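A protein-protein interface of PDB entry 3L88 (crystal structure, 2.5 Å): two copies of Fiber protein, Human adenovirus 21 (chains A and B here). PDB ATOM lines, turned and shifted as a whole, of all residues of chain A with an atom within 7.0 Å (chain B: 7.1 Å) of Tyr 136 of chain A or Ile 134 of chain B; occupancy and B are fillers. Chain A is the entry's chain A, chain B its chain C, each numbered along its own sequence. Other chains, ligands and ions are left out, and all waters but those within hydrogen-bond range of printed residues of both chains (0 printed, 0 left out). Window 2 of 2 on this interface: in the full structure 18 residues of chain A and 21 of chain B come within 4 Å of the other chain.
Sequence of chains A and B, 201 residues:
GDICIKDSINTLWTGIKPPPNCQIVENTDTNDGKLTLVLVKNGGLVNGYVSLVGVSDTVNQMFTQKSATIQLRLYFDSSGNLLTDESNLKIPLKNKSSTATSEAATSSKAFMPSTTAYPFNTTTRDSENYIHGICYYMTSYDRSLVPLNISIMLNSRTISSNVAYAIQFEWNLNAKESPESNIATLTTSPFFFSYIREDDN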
ATOM      1  N   PHE A  63      38.324  14.127  18.238  1.00  0.00           N
ATOM      2  CA  PHE A  63      38.507  13.575  19.573  1.00  0.00           C
ATOM      3  C   PHE A  63      39.977  13.590  19.989  1.00  0.00           C
ATOM      4  O   PHE A  63      40.366  12.988  20.988  1.00  0.00           O
ATOM      5  CB  PHE A  63      37.896  12.176  19.682  1.00  0.00           C
ATOM      6  CG  PHE A  63      36.391  12.174  19.705  1.00  0.00           C
ATOM      7  CD1 PHE A  63      35.683  13.365  19.708  1.00  0.00           C
ATOM      8  CD2 PHE A  63      35.686  10.985  19.756  1.00  0.00           C
ATOM      9  CE1 PHE A  63      34.300  13.368  19.731  1.00  0.00           C
ATOM     10  CE2 PHE A  63      34.300  10.980  19.779  1.00  0.00           C
ATOM     11  CZ  PHE A  63      33.608  12.174  19.766  1.00  0.00           C
ATOM     12  N   ILE A 134      22.855  10.102  27.160  1.00  0.00           N
ATOM     13  CA  ILE A 134      24.272   9.814  27.039  1.00  0.00           C
ATOM     14  C   ILE A 134      24.504   8.583  26.162  1.00  0.00           C
ATOM     15  O   ILE A 134      23.815   7.570  26.298  1.00  0.00           O
ATOM     16  CB  ILE A 134      24.913   9.597  28.425  1.00  0.00           C
ATOM     17  CG1 ILE A 134      24.724  10.841  29.301  1.00  0.00           C
ATOM     18  CG2 ILE A 134      26.393   9.257  28.288  1.00  0.00           C
ATOM     19  CD1 ILE A 134      25.361  10.731  30.678  1.00  0.00           C
ATOM     20  N   CYS A 135      25.446   8.697  25.230  1.00  0.00           N
ATOM     21  CA  CYS A 135      26.042   7.535  24.586  1.00  0.00           C
ATOM     22  C   CYS A 135      27.549   7.586  24.764  1.00  0.00           C
ATOM     23  O   CYS A 135      28.065   8.415  25.522  1.00  0.00           O
ATOM     24  CB  CYS A 135      25.672   7.477  23.103  1.00  0.00           C
ATOM     25  SG  CYS A 135      26.060   8.979  22.162  1.00  0.00           S
ATOM     26  N   TYR A 136      28.256   6.687  24.088  1.00  0.00           N
ATOM     27  CA  TYR A 136      29.642   6.414  24.453  1.00  0.00           C
ATOM     28  C   TYR A 136      30.566   6.257  23.253  1.00  0.00           C
ATOM     29  O   TYR A 136      30.160   5.781  22.190  1.00  0.00           O
ATOM     30  CB  TYR A 136      29.729   5.188  25.370  1.00  0.00           C
ATOM     31  CG  TYR A 136      28.913   5.334  26.632  1.00  0.00           C
ATOM     32  CD1 TYR A 136      27.552   5.052  26.635  1.00  0.00           C
ATOM     33  CD2 TYR A 136      29.490   5.798  27.805  1.00  0.00           C
ATOM     34  CE1 TYR A 136      26.789   5.218  27.777  1.00  0.00           C
ATOM     35  CE2 TYR A 136      28.740   5.963  28.955  1.00  0.00           C
ATOM     36  CZ  TYR A 136      27.390   5.669  28.935  1.00  0.00           C
ATOM     37  OH  TYR A 136      26.633   5.825  30.078  1.00  0.00           O
ATOM     38  N   TYR A 137      31.813   6.679  23.438  1.00  0.00           N
ATOM     39  CA  TYR A 137      32.861   6.451  22.460  1.00  0.00           C
ATOM     40  C   TYR A 137      33.882   5.483  23.037  1.00  0.00           C
ATOM     41  O   TYR A 137      34.297   5.623  24.190  1.00  0.00           O
ATOM     42  CB  TYR A 137      33.531   7.778  22.087  1.00  0.00           C
ATOM     43  CG  TYR A 137      34.790   7.625  21.258  1.00  0.00           C
ATOM     44  CD1 TYR A 137      34.721   7.291  19.913  1.00  0.00           C
ATOM     45  CD2 TYR A 137      36.051   7.824  21.822  1.00  0.00           C
ATOM     46  CE1 TYR A 137      35.873   7.145  19.154  1.00  0.00           C
ATOM     47  CE2 TYR A 137      37.207   7.683  21.070  1.00  0.00           C
ATOM     48  CZ  TYR A 137      37.112   7.339  19.741  1.00  0.00           C
ATOM     49  OH  TYR A 137      38.262   7.197  19.003  1.00  0.00           O
ATOM     50  N   MET A 138      34.261   4.487  22.241  1.00  0.00           N
ATOM     51  CA  MET A 138      35.317   3.549  22.626  1.00  0.00           C
ATOM     52  C   MET A 138      36.671   4.031  22.104  1.00  0.00           C
ATOM     53  O   MET A 138      36.877   4.133  20.893  1.00  0.00           O
ATOM     54  CB  MET A 138      35.016   2.155  22.073  1.00  0.00           C
ATOM     55  CG  MET A 138      34.087   1.322  22.934  1.00  0.00           C
ATOM     56  SD  MET A 138      33.861  -0.350  22.291  1.00  0.00           S
ATOM     57  CE  MET A 138      35.568  -0.852  22.061  1.00  0.00           C
ATOM     58  N   LEU A 145      35.584   3.528  27.811  1.00  0.00           N
ATOM     59  CA  LEU A 145      34.361   4.231  27.415  1.00  0.00           C
ATOM     60  C   LEU A 145      34.417   5.715  27.770  1.00  0.00           C
ATOM     61  O   LEU A 145      34.585   6.078  28.931  1.00  0.00           O
ATOM     62  CB  LEU A 145      33.140   3.594  28.077  1.00  0.00           C
ATOM     63  CG  LEU A 145      32.379   2.537  27.276  1.00  0.00           C
ATOM     64  CD1 LEU A 145      33.318   1.744  26.392  1.00  0.00           C
ATOM     65  CD2 LEU A 145      31.611   1.617  28.209  1.00  0.00           C
ATOM     66  N   VAL A 146      34.266   6.570  26.766  1.00  0.00           N
ATOM     67  CA  VAL A 146      34.147   8.003  27.001  1.00  0.00           C
ATOM     68  C   VAL A 146      32.717   8.478  26.763  1.00  0.00           C
ATOM     69  O   VAL A 146      32.145   8.223  25.709  1.00  0.00           O
ATOM     70  CB  VAL A 146      35.118   8.801  26.112  1.00  0.00           C
ATOM     71  CG1 VAL A 146      34.912  10.298  26.302  1.00  0.00           C
ATOM     72  CG2 VAL A 146      36.558   8.407  26.419  1.00  0.00           C
ATOM     73  N   PRO A 147      32.125   9.138  27.768  1.00  0.00           N
ATOM     74  CA  PRO A 147      30.738   9.611  27.722  1.00  0.00           C
ATOM     75  C   PRO A 147      30.552  10.758  26.738  1.00  0.00           C
ATOM     76  O   PRO A 147      31.342  11.701  26.726  1.00  0.00           O
ATOM     77  CB  PRO A 147      30.487  10.123  29.145  1.00  0.00           C
ATOM     78  CG  PRO A 147      31.626   9.611  29.973  1.00  0.00           C
ATOM     79  CD  PRO A 147      32.778   9.461  29.047  1.00  0.00           C
ATOM     80  N   LEU A 148      29.499  10.682  25.933  1.00  0.00           N
ATOM     81  CA  LEU A 148      29.101  11.798  25.079  1.00  0.00           C
ATOM     82  C   LEU A 148      27.681  12.243  25.411  1.00  0.00           C
ATOM     83  O   LEU A 148      26.747  11.442  25.385  1.00  0.00           O
ATOM     84  CB  LEU A 148      29.178  11.394  23.607  1.00  0.00           C
ATOM     85  CG  LEU A 148      30.544  10.951  23.072  1.00  0.00           C
ATOM     86  CD1 LEU A 148      30.412  10.373  21.668  1.00  0.00           C
ATOM     87  CD2 LEU A 148      31.537  12.106  23.084  1.00  0.00           C
ATOM     88  N   TRP A 171      25.998  15.898  19.539  1.00  0.00           N
ATOM     89  CA  TRP A 171      26.884  15.181  20.447  1.00  0.00           C
ATOM     90  C   TRP A 171      27.923  16.139  21.030  1.00  0.00           C
ATOM     91  O   TRP A 171      28.517  16.946  20.309  1.00  0.00           O
ATOM     92  CB  TRP A 171      27.597  14.036  19.720  1.00  0.00           C
ATOM     93  CG  TRP A 171      26.698  12.906  19.292  1.00  0.00           C
ATOM     94  CD1 TRP A 171      26.467  11.742  19.966  1.00  0.00           C
ATOM     95  CD2 TRP A 171      25.948  12.819  18.072  1.00  0.00           C
ATOM     96  NE1 TRP A 171      25.603  10.948  19.255  1.00  0.00           N
ATOM     97  CE2 TRP A 171      25.272  11.583  18.087  1.00  0.00           C
ATOM     98  CE3 TRP A 171      25.773  13.672  16.978  1.00  0.00           C
ATOM     99  CZ2 TRP A 171      24.429  11.177  17.046  1.00  0.00           C
ATOM    100  CZ3 TRP A 171      24.933  13.274  15.947  1.00  0.00           C
ATOM    101  CH2 TRP A 171      24.278  12.032  15.985  1.00  0.00           C
ATOM    102  N   THR A 187      33.230   6.979  16.289  1.00  0.00           N
ATOM    103  CA  THR A 187      31.965   6.261  16.326  1.00  0.00           C
ATOM    104  C   THR A 187      31.205   6.629  17.591  1.00  0.00           C
ATOM    105  O   THR A 187      31.799   6.769  18.655  1.00  0.00           O
ATOM    106  CB  THR A 187      32.171   4.736  16.330  1.00  0.00           C
ATOM    107  OG1 THR A 187      32.727   4.335  17.588  1.00  0.00           O
ATOM    108  CG2 THR A 187      33.096   4.310  15.208  1.00  0.00           C
ATOM    109  N   THR A 188      29.890   6.780  17.471  1.00  0.00           N
ATOM    110  CA  THR A 188      29.035   6.971  18.641  1.00  0.00           C
ATOM    111  C   THR A 188      28.115   5.768  18.823  1.00  0.00           C
ATOM    112  O   THR A 188      27.408   5.367  17.897  1.00  0.00           O
ATOM    113  CB  THR A 188      28.172   8.244  18.520  1.00  0.00           C
ATOM    114  OG1 THR A 188      27.190   8.060  17.489  1.00  0.00           O
ATOM    115  CG2 THR A 188      29.040   9.463  18.211  1.00  0.00           C
ATOM    116  N   SER A 189      28.118   5.196  20.021  1.00  0.00           N
ATOM    117  CA  SER A 189      27.253   4.059  20.299  1.00  0.00           C
ATOM    118  C   SER A 189      25.789   4.451  20.130  1.00  0.00           C
ATOM    119  O   SER A 189      25.426   5.604  20.341  1.00  0.00           O
ATOM    120  CB  SER A 189      27.524   3.485  21.695  1.00  0.00           C
ATOM    121  OG  SER A 189      27.194   4.407  22.716  1.00  0.00           O
ATOM    122  N   PRO A 190      24.950   3.499  19.702  1.00  0.00           N
ATOM    123  CA  PRO A 190      23.562   3.800  19.365  1.00  0.00           C
ATOM    124  C   PRO A 190      22.824   4.448  20.527  1.00  0.00           C
ATOM    125  O   PRO A 190      22.947   4.006  21.661  1.00  0.00           O
ATOM    126  CB  PRO A 190      22.964   2.422  19.073  1.00  0.00           C
ATOM    127  CG  PRO A 190      24.127   1.582  18.683  1.00  0.00           C
ATOM    128  CD  PRO A 190      25.268   2.074  19.513  1.00  0.00           C
ATOM    129  N   ILE B 131      26.354  -1.981  21.920  1.00  0.00           N
ATOM    130  CA  ILE B 131      25.476  -1.032  22.594  1.00  0.00           C
ATOM    131  C   ILE B 131      25.949  -0.835  24.028  1.00  0.00           C
ATOM    132  O   ILE B 131      26.333  -1.790  24.701  1.00  0.00           O
ATOM    133  CB  ILE B 131      24.014  -1.514  22.608  1.00  0.00           C
ATOM    134  CG1 ILE B 131      23.442  -1.542  21.187  1.00  0.00           C
ATOM    135  CG2 ILE B 131      23.169  -0.633  23.512  1.00  0.00           C
ATOM    136  CD1 ILE B 131      22.182  -2.379  21.062  1.00  0.00           C
ATOM    137  N   HIS B 132      25.945   0.413  24.482  1.00  0.00           N
ATOM    138  CA  HIS B 132      26.422   0.736  25.819  1.00  0.00           C
ATOM    139  C   HIS B 132      25.397   1.548  26.597  1.00  0.00           C
ATOM    140  O   HIS B 132      24.677   2.365  26.031  1.00  0.00           O
ATOM    141  CB  HIS B 132      27.735   1.505  25.742  1.00  0.00           C
ATOM    142  CG  HIS B 132      28.860   0.721  25.148  1.00  0.00           C
ATOM    143  ND1 HIS B 132      29.446   1.057  23.947  1.00  0.00           N
ATOM    144  CD2 HIS B 132      29.521  -0.371  25.598  1.00  0.00           C
ATOM    145  CE1 HIS B 132      30.419   0.205  23.681  1.00  0.00           C
ATOM    146  NE2 HIS B 132      30.486  -0.671  24.667  1.00  0.00           N
ATOM    147  N   GLY B 133      25.345   1.332  27.905  1.00  0.00           N
ATOM    148  CA  GLY B 133      24.399   2.051  28.746  1.00  0.00           C
ATOM    149  C   GLY B 133      24.582   1.742  30.215  1.00  0.00           C
ATOM    150  O   GLY B 133      25.590   1.156  30.616  1.00  0.00           O
ATOM    151  N   ILE B 134      23.601   2.132  31.023  1.00  0.00           N
ATOM    152  CA  ILE B 134      23.699   1.973  32.461  1.00  0.00           C
ATOM    153  C   ILE B 134      22.391   1.451  33.035  1.00  0.00           C
ATOM    154  O   ILE B 134      21.315   1.924  32.677  1.00  0.00           O
ATOM    155  CB  ILE B 134      24.067   3.302  33.145  1.00  0.00           C
ATOM    156  CG1 ILE B 134      25.413   3.814  32.626  1.00  0.00           C
ATOM    157  CG2 ILE B 134      24.110   3.127  34.650  1.00  0.00           C
ATOM    158  CD1 ILE B 134      25.901   5.079  33.320  1.00  0.00           C
ATOM    159  N   CYS B 135      22.485   0.448  33.902  1.00  0.00           N
ATOM    160  CA  CYS B 135      21.384   0.111  34.795  1.00  0.00           C
ATOM    161  C   CYS B 135      21.867   0.135  36.240  1.00  0.00           C
ATOM    162  O   CYS B 135      22.979   0.577  36.517  1.00  0.00           O
ATOM    163  CB  CYS B 135      20.784  -1.253  34.441  1.00  0.00           C
ATOM    164  SG  CYS B 135      21.987  -2.578  34.274  1.00  0.00           S
ATOM    165  N   TYR B 136      21.036  -0.338  37.162  1.00  0.00           N
ATOM    166  CA  TYR B 136      21.252  -0.033  38.570  1.00  0.00           C
ATOM    167  C   TYR B 136      21.013  -1.212  39.497  1.00  0.00           C
ATOM    168  O   TYR B 136      20.166  -2.069  39.231  1.00  0.00           O
ATOM    169  CB  TYR B 136      20.403   1.167  38.998  1.00  0.00           C
ATOM    170  CG  TYR B 136      20.706   2.417  38.208  1.00  0.00           C
ATOM    171  CD1 TYR B 136      20.097   2.646  36.981  1.00  0.00           C
ATOM    172  CD2 TYR B 136      21.642   3.339  38.659  1.00  0.00           C
ATOM    173  CE1 TYR B 136      20.387   3.778  36.237  1.00  0.00           C
ATOM    174  CE2 TYR B 136      21.931   4.477  37.927  1.00  0.00           C
ATOM    175  CZ  TYR B 136      21.300   4.689  36.719  1.00  0.00           C
ATOM    176  OH  TYR B 136      21.603   5.811  35.992  1.00  0.00           O
ATOM    177  N   VAL B 146      23.332   1.685  42.947  1.00  0.00           N
ATOM    178  CA  VAL B 146      24.683   1.514  42.435  1.00  0.00           C
ATOM    179  C   VAL B 146      24.658   1.288  40.923  1.00  0.00           C
ATOM    180  O   VAL B 146      23.962   0.394  40.435  1.00  0.00           O
ATOM    181  CB  VAL B 146      25.411   0.345  43.133  1.00  0.00           C
ATOM    182  CG1 VAL B 146      26.785   0.134  42.521  1.00  0.00           C
ATOM    183  CG2 VAL B 146      25.518   0.603  44.632  1.00  0.00           C
ATOM    184  N   PRO B 147      25.392   2.131  40.177  1.00  0.00           N
ATOM    185  CA  PRO B 147      25.422   2.090  38.720  1.00  0.00           C
ATOM    186  C   PRO B 147      26.137   0.847  38.206  1.00  0.00           C
ATOM    187  O   PRO B 147      27.200   0.481  38.717  1.00  0.00           O
ATOM    188  CB  PRO B 147      26.227   3.342  38.338  1.00  0.00           C
ATOM    189  CG  PRO B 147      26.342   4.160  39.594  1.00  0.00           C
ATOM    190  CD  PRO B 147      26.250   3.196  40.721  1.00  0.00           C
ATOM    191  N   LEU B 148      25.562   0.217  37.186  1.00  0.00           N
ATOM    192  CA  LEU B 148      26.213  -0.886  36.502  1.00  0.00           C
ATOM    193  C   LEU B 148      26.349  -0.576  35.016  1.00  0.00           C
ATOM    194  O   LEU B 148      25.350  -0.370  34.320  1.00  0.00           O
ATOM    195  CB  LEU B 148      25.404  -2.170  36.673  1.00  0.00           C
ATOM    196  CG  LEU B 148      25.197  -2.672  38.098  1.00  0.00           C
ATOM    197  CD1 LEU B 148      24.204  -3.826  38.088  1.00  0.00           C
ATOM    198  CD2 LEU B 148      26.526  -3.097  38.702  1.00  0.00           C
ATOM    199  N   ASN B 149      27.585  -0.555  34.529  1.00  0.00           N
ATOM    200  CA  ASN B 149      27.820  -0.421  33.103  1.00  0.00           C
ATOM    201  C   ASN B 149      27.342  -1.667  32.380  1.00  0.00           C
ATOM    202  O   ASN B 149      27.780  -2.777  32.691  1.00  0.00           O
ATOM    203  CB  ASN B 149      29.304  -0.183  32.833  1.00  0.00           C
ATOM    204  CG  ASN B 149      29.858   0.983  33.635  1.00  0.00           C
ATOM    205  OD1 ASN B 149      29.397   2.118  33.506  1.00  0.00           O
ATOM    206  ND2 ASN B 149      30.840   0.705  34.482  1.00  0.00           N
ATOM    207  N   ILE B 150      26.407  -1.489  31.450  1.00  0.00           N
ATOM    208  CA  ILE B 150      25.927  -2.598  30.640  1.00  0.00           C
ATOM    209  C   ILE B 150      26.334  -2.388  29.193  1.00  0.00           C
ATOM    210  O   ILE B 150      26.148  -1.306  28.637  1.00  0.00           O
ATOM    211  CB  ILE B 150      24.393  -2.753  30.724  1.00  0.00           C
ATOM    212  CG1 ILE B 150      23.887  -3.703  29.631  1.00  0.00           C
ATOM    213  CG2 ILE B 150      23.717  -1.401  30.576  1.00  0.00           C
ATOM    214  CD1 ILE B 150      23.839  -5.146  30.039  1.00  0.00           C
ATOM    215  N   SER B 151      26.916  -3.420  28.593  1.00  0.00           N
ATOM    216  CA  SER B 151      27.234  -3.385  27.176  1.00  0.00           C
ATOM    217  C   SER B 151      26.728  -4.636  26.476  1.00  0.00           C
ATOM    218  O   SER B 151      26.855  -5.748  26.982  1.00  0.00           O
ATOM    219  CB  SER B 151      28.734  -3.211  26.955  1.00  0.00           C
ATOM    220  OG  SER B 151      29.421  -4.414  27.215  1.00  0.00           O
ATOM    221  N   SER B 189      18.440  -3.801  37.396  1.00  0.00           N
ATOM    222  CA  SER B 189      17.242  -3.124  36.911  1.00  0.00           C
ATOM    223  C   SER B 189      17.152  -3.212  35.386  1.00  0.00           C
ATOM    224  O   SER B 189      18.171  -3.242  34.696  1.00  0.00           O
ATOM    225  CB  SER B 189      17.201  -1.667  37.378  1.00  0.00           C
ATOM    226  OG  SER B 189      18.220  -0.901  36.763  1.00  0.00           O
ATOM    227  N   PRO B 190      15.923  -3.281  34.861  1.00  0.00           N
ATOM    228  CA  PRO B 190      15.736  -3.551  33.442  1.00  0.00           C
ATOM    229  C   PRO B 190      16.511  -2.562  32.577  1.00  0.00           C
ATOM    230  O   PRO B 190      16.553  -1.368  32.878  1.00  0.00           O
ATOM    231  CB  PRO B 190      14.228  -3.372  33.250  1.00  0.00           C
ATOM    232  CG  PRO B 190      13.643  -3.645  34.588  1.00  0.00           C
ATOM    233  CD  PRO B 190      14.644  -3.125  35.574  1.00  0.00           C
ATOM    234  N   PHE B 191      17.146  -3.067  31.525  1.00  0.00           N
ATOM    235  CA  PHE B 191      17.797  -2.207  30.548  1.00  0.00           C
ATOM    236  C   PHE B 191      17.067  -2.300  29.215  1.00  0.00           C
ATOM    237  O   PHE B 191      16.684  -3.387  28.788  1.00  0.00           O
ATOM    238  CB  PHE B 191      19.266  -2.599  30.387  1.00  0.00           C
ATOM    239  CG  PHE B 191      20.010  -1.759  29.391  1.00  0.00           C
ATOM    240  CD1 PHE B 191      20.188  -0.398  29.604  1.00  0.00           C
ATOM    241  CD2 PHE B 191      20.555  -2.329  28.256  1.00  0.00           C
ATOM    242  CE1 PHE B 191      20.889   0.386  28.692  1.00  0.00           C
ATOM    243  CE2 PHE B 191      21.265  -1.561  27.347  1.00  0.00           C
ATOM    244  CZ  PHE B 191      21.425  -0.197  27.560  1.00  0.00           C
ATOM    245  N   PHE B 192      16.845  -1.151  28.584  1.00  0.00           N
ATOM    246  CA  PHE B 192      16.105  -1.092  27.328  1.00  0.00           C
ATOM    247  C   PHE B 192      17.037  -0.811  26.154  1.00  0.00           C
ATOM    248  O   PHE B 192      17.933   0.026  26.243  1.00  0.00           O
ATOM    249  CB  PHE B 192      15.013  -0.017  27.388  1.00  0.00           C
ATOM    250  CG  PHE B 192      14.311   0.064  28.711  1.00  0.00           C
ATOM    251  CD1 PHE B 192      14.345   1.232  29.451  1.00  0.00           C
ATOM    252  CD2 PHE B 192      13.616  -1.026  29.216  1.00  0.00           C
ATOM    253  CE1 PHE B 192      13.701   1.321  30.672  1.00  0.00           C
ATOM    254  CE2 PHE B 192      12.969  -0.950  30.441  1.00  0.00           C
ATOM    255  CZ  PHE B 192      13.007   0.229  31.167  1.00  0.00           C
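The backbone NH (N) of Tyr 136 of chain A is in hydrogen-bond range of the side-chain hydroxyl (OG) of Ser 189 of chain A, 2.9 Å away.
Tyr 136 of chain A touches His 132 of chain B (CD1 to CB, 3.7 Å).
OH of Tyr 136 of chain A touches CD1 of Ile 134 of chain B, at 3.4 Å.
SD of Met 138 of chain A touches CE1 of His 132 of chain B, at 3.8 Å.
CD2 of Leu 145 of chain A touches CD2 of His 132 of chain B, 3.9 Å away.
Ser 189 of chain A touches His 132 of chain B (CB to ND1, 3.8 Å).
Tyr 136 of chain A touches just these residues of chain B: His 132 and Ile 134.
Printed residues of chain A within 4 Å of Ile 134 of chain B: Tyr 136 (3.4 Å).
Printed residues of chain A within 4 Å of His 132 of chain B: Tyr 136, Met 138, Leu 145 and Ser 189.
Printed residues of chain B within 4 Å of Met 138 of chain A: His 132.
Phe 191 of chain B touches none of the printed residues of chain A.
Ser 189 of chain B touches none of the printed residues of chain A.
The nearest residue of chain B that does not touch Tyr 136 of chain A is Gly 133 of chain B (4.1 Å).
Tyr 136 of chain A touches Ile 134 of chain B, but with the chains exchanged Ile 134 of chain A does not touch Tyr 136 of chain B (8.2 Å).
8 positions are printed for both chains.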
